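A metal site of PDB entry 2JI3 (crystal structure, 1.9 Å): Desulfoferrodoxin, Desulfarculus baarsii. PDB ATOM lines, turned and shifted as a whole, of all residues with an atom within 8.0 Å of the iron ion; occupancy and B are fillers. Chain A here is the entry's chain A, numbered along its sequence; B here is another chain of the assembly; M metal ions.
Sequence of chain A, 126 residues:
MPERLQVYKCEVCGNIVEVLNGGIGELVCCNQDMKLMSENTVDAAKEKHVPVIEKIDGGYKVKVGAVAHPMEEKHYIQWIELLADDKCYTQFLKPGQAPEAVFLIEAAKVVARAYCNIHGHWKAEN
SG of Cys 13 binds the iron ion (2.2 Å). The iron ion is bound by the side-chain sulfur (SG) of Cys 29, at 2.2 Å. SG of Cys 10 is bound to the iron ion. The side-chain sulfur (SG) of Cys 30 binds the iron ion, at 2.4 Å.
Of the 20 residues printed, 4 come within 4 Å of the iron ion. The nearest printed residue that does not touch the iron ion is Gly 25 of chain B (4.02 Å).
SG of Cys 13 lies close to N of Gly 25 of chain B (3.4 Å). The side-chain sulfur (SG) of Cys 13 lies close to the side-chain amide nitrogen (ND2) of Asn 15, at 3.4 Å. The side-chain sulfur (SG) of Cys 29 lies close to the side-chain amide nitrogen (ND2) of Asn 15, at 3.4 Å. The backbone carbonyl oxygen (O) of Asn 15 lies within hydrogen-bond range of the backbone NH (N) of Cys 10, at 2.9 Å. SG of Cys 10 lies close to N of Val 12 (3.5 Å).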
ATOM      1  N   LYS A   9      -3.352  22.024   1.459  1.00  0.00           N
ATOM      2  CA  LYS A   9      -4.429  22.934   1.113  1.00  0.00           C
ATOM      3  C   LYS A   9      -4.036  24.394   1.205  1.00  0.00           C
ATOM      4  O   LYS A   9      -3.293  24.802   2.116  1.00  0.00           O
ATOM      5  CB  LYS A   9      -5.629  22.720   2.043  1.00  0.00           C
ATOM      6  CG  LYS A   9      -6.758  23.737   1.845  1.00  0.00           C
ATOM      7  CD  LYS A   9      -7.864  23.606   2.882  1.00  0.00           C
ATOM      8  CE  LYS A   9      -8.972  24.631   2.616  1.00  0.00           C
ATOM      9  NZ  LYS A   9     -10.127  24.503   3.567  1.00  0.00           N
ATOM     10  N   CYS A  10      -4.528  25.180   0.249  1.00  0.00           N
ATOM     11  CA  CYS A  10      -4.314  26.624   0.258  1.00  0.00           C
ATOM     12  C   CYS A  10      -5.566  27.133   0.975  1.00  0.00           C
ATOM     13  O   CYS A  10      -6.672  26.963   0.483  1.00  0.00           O
ATOM     14  CB  CYS A  10      -4.296  27.196  -1.151  1.00  0.00           C
ATOM     15  SG  CYS A  10      -4.228  29.010  -1.137  1.00  0.00           S
ATOM     16  N   GLU A  11      -5.378  27.743   2.140  1.00  0.00           N
ATOM     17  CA  GLU A  11      -6.514  28.239   2.896  1.00  0.00           C
ATOM     18  C   GLU A  11      -7.131  29.498   2.287  1.00  0.00           C
ATOM     19  O   GLU A  11      -8.195  29.942   2.705  1.00  0.00           O
ATOM     20  CB  GLU A  11      -6.113  28.495   4.350  1.00  0.00           C
ATOM     21  CG  GLU A  11      -5.708  27.220   5.083  1.00  0.00           C
ATOM     22  CD  GLU A  11      -5.292  27.469   6.526  1.00  0.00           C
ATOM     23  OE1 GLU A  11      -4.278  28.160   6.743  1.00  0.00           O
ATOM     24  OE2 GLU A  11      -5.985  26.971   7.445  1.00  0.00           O
ATOM     25  N   VAL A  12      -6.456  30.071   1.293  1.00  0.00           N
ATOM     26  CA  VAL A  12      -6.964  31.264   0.623  1.00  0.00           C
ATOM     27  C   VAL A  12      -7.927  30.898  -0.503  1.00  0.00           C
ATOM     28  O   VAL A  12      -9.117  31.191  -0.407  1.00  0.00           O
ATOM     29  CB  VAL A  12      -5.824  32.145   0.050  1.00  0.00           C
ATOM     30  CG1 VAL A  12      -6.405  33.269  -0.782  1.00  0.00           C
ATOM     31  CG2 VAL A  12      -5.001  32.749   1.190  1.00  0.00           C
ATOM     32  N   CYS A  13      -7.430  30.258  -1.556  1.00  0.00           N
ATOM     33  CA  CYS A  13      -8.292  29.898  -2.695  1.00  0.00           C
ATOM     34  C   CYS A  13      -8.917  28.513  -2.627  1.00  0.00           C
ATOM     35  O   CYS A  13      -9.773  28.167  -3.441  1.00  0.00           O
ATOM     36  CB  CYS A  13      -7.510  30.019  -3.999  1.00  0.00           C
ATOM     37  SG  CYS A  13      -6.218  28.762  -4.215  1.00  0.00           S
ATOM     38  N   GLY A  14      -8.483  27.681  -1.682  1.00  0.00           N
ATOM     39  CA  GLY A  14      -9.095  26.370  -1.557  1.00  0.00           C
ATOM     40  C   GLY A  14      -8.503  25.229  -2.361  1.00  0.00           C
ATOM     41  O   GLY A  14      -9.063  24.140  -2.386  1.00  0.00           O
ATOM     42  N   ASN A  15      -7.389  25.478  -3.050  1.00  0.00           N
ATOM     43  CA  ASN A  15      -6.741  24.403  -3.806  1.00  0.00           C
ATOM     44  C   ASN A  15      -6.322  23.320  -2.822  1.00  0.00           C
ATOM     45  O   ASN A  15      -5.850  23.612  -1.730  1.00  0.00           O
ATOM     46  CB  ASN A  15      -5.453  24.889  -4.491  1.00  0.00           C
ATOM     47  CG  ASN A  15      -5.693  25.553  -5.840  1.00  0.00           C
ATOM     48  OD1 ASN A  15      -6.665  25.259  -6.537  1.00  0.00           O
ATOM     49  ND2 ASN A  15      -4.778  26.438  -6.212  1.00  0.00           N
ATOM     50  N   ILE A  16      -6.515  22.056  -3.210  1.00  0.00           N
ATOM     51  CA  ILE A  16      -6.082  20.943  -2.386  1.00  0.00           C
ATOM     52  C   ILE A  16      -5.375  19.983  -3.338  1.00  0.00           C
ATOM     53  O   ILE A  16      -5.912  19.621  -4.380  1.00  0.00           O
ATOM     54  CB  ILE A  16      -7.247  20.187  -1.714  1.00  0.00           C
ATOM     55  CG1 ILE A  16      -7.973  21.109  -0.726  1.00  0.00           C
ATOM     56  CG2 ILE A  16      -6.705  18.960  -0.973  1.00  0.00           C
ATOM     57  CD1 ILE A  16      -9.140  20.451   0.021  1.00  0.00           C
ATOM     58  N   VAL A  28       3.574  26.315  -2.257  1.00  0.00           N
ATOM     59  CA  VAL A  28       3.002  27.612  -1.964  1.00  0.00           C
ATOM     60  C   VAL A  28       1.839  27.929  -2.896  1.00  0.00           C
ATOM     61  O   VAL A  28       1.764  27.424  -4.014  1.00  0.00           O
ATOM     62  CB  VAL A  28       4.090  28.718  -2.106  1.00  0.00           C
ATOM     63  CG1 VAL A  28       3.470  30.111  -1.941  1.00  0.00           C
ATOM     64  CG2 VAL A  28       5.176  28.506  -1.059  1.00  0.00           C
ATOM     65  N   CYS A  29       0.913  28.753  -2.401  1.00  0.00           N
ATOM     66  CA  CYS A  29      -0.238  29.156  -3.194  1.00  0.00           C
ATOM     67  C   CYS A  29      -0.799  30.431  -2.581  1.00  0.00           C
ATOM     68  O   CYS A  29      -0.814  30.601  -1.359  1.00  0.00           O
ATOM     69  CB  CYS A  29      -1.297  28.051  -3.212  1.00  0.00           C
ATOM     70  SG  CYS A  29      -2.676  28.331  -4.356  1.00  0.00           S
ATOM     71  N   CYS A  30      -1.252  31.335  -3.438  1.00  0.00           N
ATOM     72  CA  CYS A  30      -1.797  32.605  -2.999  1.00  0.00           C
ATOM     73  C   CYS A  30      -0.870  33.314  -2.006  1.00  0.00           C
ATOM     74  O   CYS A  30      -1.323  33.867  -1.000  1.00  0.00           O
ATOM     75  CB  CYS A  30      -3.182  32.384  -2.369  1.00  0.00           C
ATOM     76  SG  CYS A  30      -4.400  31.790  -3.541  1.00  0.00           S
ATOM     77  N   ASN A  31       0.421  33.271  -2.297  1.00  0.00           N
ATOM     78  CA  ASN A  31       1.441  33.935  -1.476  1.00  0.00           C
ATOM     79  C   ASN A  31       1.675  33.408  -0.065  1.00  0.00           C
ATOM     80  O   ASN A  31       2.284  34.096   0.747  1.00  0.00           O
ATOM     81  CB  ASN A  31       1.155  35.438  -1.405  1.00  0.00           C
ATOM     82  CG  ASN A  31       1.286  36.107  -2.763  1.00  0.00           C
ATOM     83  OD1 ASN A  31       0.504  36.997  -3.093  1.00  0.00           O
ATOM     84  ND2 ASN A  31       2.285  35.693  -3.541  1.00  0.00           N
ATOM     85  N   GLN A  32       1.194  32.206   0.220  1.00  0.00           N
ATOM     86  CA  GLN A  32       1.420  31.632   1.542  1.00  0.00           C
ATOM     87  C   GLN A  32       1.664  30.115   1.460  1.00  0.00           C
ATOM     88  O   GLN A  32       1.264  29.468   0.486  1.00  0.00           O
ATOM     89  CB  GLN A  32       0.251  31.946   2.484  1.00  0.00           C
ATOM     90  CG  GLN A  32      -1.079  31.301   2.171  1.00  0.00           C
ATOM     91  CD  GLN A  32      -2.184  31.778   3.110  1.00  0.00           C
ATOM     92  OE1 GLN A  32      -3.104  31.028   3.456  1.00  0.00           O
ATOM     93  NE2 GLN A  32      -2.092  33.035   3.511  1.00  0.00           N
ATOM     94  N   MET A  34       1.282  26.307   1.690  1.00  0.00           N
ATOM     95  CA  MET A  34       0.105  25.467   1.697  1.00  0.00           C
ATOM     96  C   MET A  34       0.152  24.695   3.002  1.00  0.00           C
ATOM     97  O   MET A  34       1.229  24.299   3.454  1.00  0.00           O
ATOM     98  CB  MET A  34       0.088  24.516   0.504  1.00  0.00           C
ATOM     99  CG  MET A  34      -0.045  25.205  -0.843  1.00  0.00           C
ATOM    100  SD  MET A  34      -0.219  24.029  -2.206  1.00  0.00           S
ATOM    101  CE  MET A  34      -1.964  23.676  -2.118  1.00  0.00           C
ATOM    102  N   PRO B   2      -6.242  25.718 -11.103  1.00  0.00           N
ATOM    103  CA  PRO B   2      -6.119  24.270 -11.376  1.00  0.00           C
ATOM    104  C   PRO B   2      -7.428  23.518 -11.209  1.00  0.00           C
ATOM    105  O   PRO B   2      -8.371  23.986 -10.553  1.00  0.00           O
ATOM    106  CB  PRO B   2      -5.069  23.731 -10.412  1.00  0.00           C
ATOM    107  CG  PRO B   2      -5.104  24.764  -9.307  1.00  0.00           C
ATOM    108  CD  PRO B   2      -5.316  26.092 -10.032  1.00  0.00           C
ATOM    109  N   GLY B  23      -9.184  25.261  -7.641  1.00  0.00           N
ATOM    110  CA  GLY B  23      -9.247  26.602  -7.070  1.00  0.00           C
ATOM    111  C   GLY B  23      -8.679  27.562  -8.105  1.00  0.00           C
ATOM    112  O   GLY B  23      -8.230  27.121  -9.157  1.00  0.00           O
ATOM    113  N   ILE B  24      -8.675  28.860  -7.813  1.00  0.00           N
ATOM    114  CA  ILE B  24      -8.163  29.833  -8.770  1.00  0.00           C
ATOM    115  C   ILE B  24      -6.675  30.148  -8.638  1.00  0.00           C
ATOM    116  O   ILE B  24      -6.046  30.630  -9.576  1.00  0.00           O
ATOM    117  CB  ILE B  24      -8.929  31.160  -8.668  1.00  0.00           C
ATOM    118  CG1 ILE B  24      -8.758  31.746  -7.257  1.00  0.00           C
ATOM    119  CG2 ILE B  24     -10.394  30.942  -8.997  1.00  0.00           C
ATOM    120  CD1 ILE B  24      -9.450  33.057  -7.045  1.00  0.00           C
ATOM    121  N   GLY B  25      -6.094  29.877  -7.472  1.00  0.00           N
ATOM    122  CA  GLY B  25      -4.690  30.175  -7.280  1.00  0.00           C
ATOM    123  C   GLY B  25      -3.726  29.309  -8.056  1.00  0.00           C
ATOM    124  O   GLY B  25      -4.018  28.157  -8.383  1.00  0.00           O
ATOM    125  N   GLU B  26      -2.566  29.873  -8.389  1.00  0.00           N
ATOM    126  CA  GLU B  26      -1.559  29.107  -9.119  1.00  0.00           C
ATOM    127  C   GLU B  26      -0.608  28.434  -8.145  1.00  0.00           C
ATOM    128  O   GLU B  26      -0.074  29.068  -7.235  1.00  0.00           O
ATOM    129  CB  GLU B  26      -0.753  30.018 -10.054  1.00  0.00           C
ATOM    130  CG  GLU B  26      -1.496  30.450 -11.310  1.00  0.00           C
ATOM    131  CD  GLU B  26      -2.098  31.839 -11.191  1.00  0.00           C
ATOM    132  OE1 GLU B  26      -2.806  32.261 -12.141  1.00  0.00           O
ATOM    133  OE2 GLU B  26      -1.857  32.526 -10.170  1.00  0.00           O
ATOM    134  N   LEU B  27      -0.416  27.129  -8.331  1.00  0.00           N
ATOM    135  CA  LEU B  27       0.485  26.365  -7.471  1.00  0.00           C
ATOM    136  C   LEU B  27       1.918  26.821  -7.743  1.00  0.00           C
ATOM    137  O   LEU B  27       2.346  26.938  -8.907  1.00  0.00           O
ATOM    138  CB  LEU B  27       0.323  24.864  -7.768  1.00  0.00           C
ATOM    139  CG  LEU B  27      -1.084  24.327  -7.515  1.00  0.00           C
ATOM    140  CD1 LEU B  27      -1.231  22.958  -8.133  1.00  0.00           C
ATOM    141  CD2 LEU B  27      -1.361  24.293  -6.022  1.00  0.00           C
HETATM  142 FE    FE M   1      -4.320  29.447  -3.344  1.00  0.00          FE
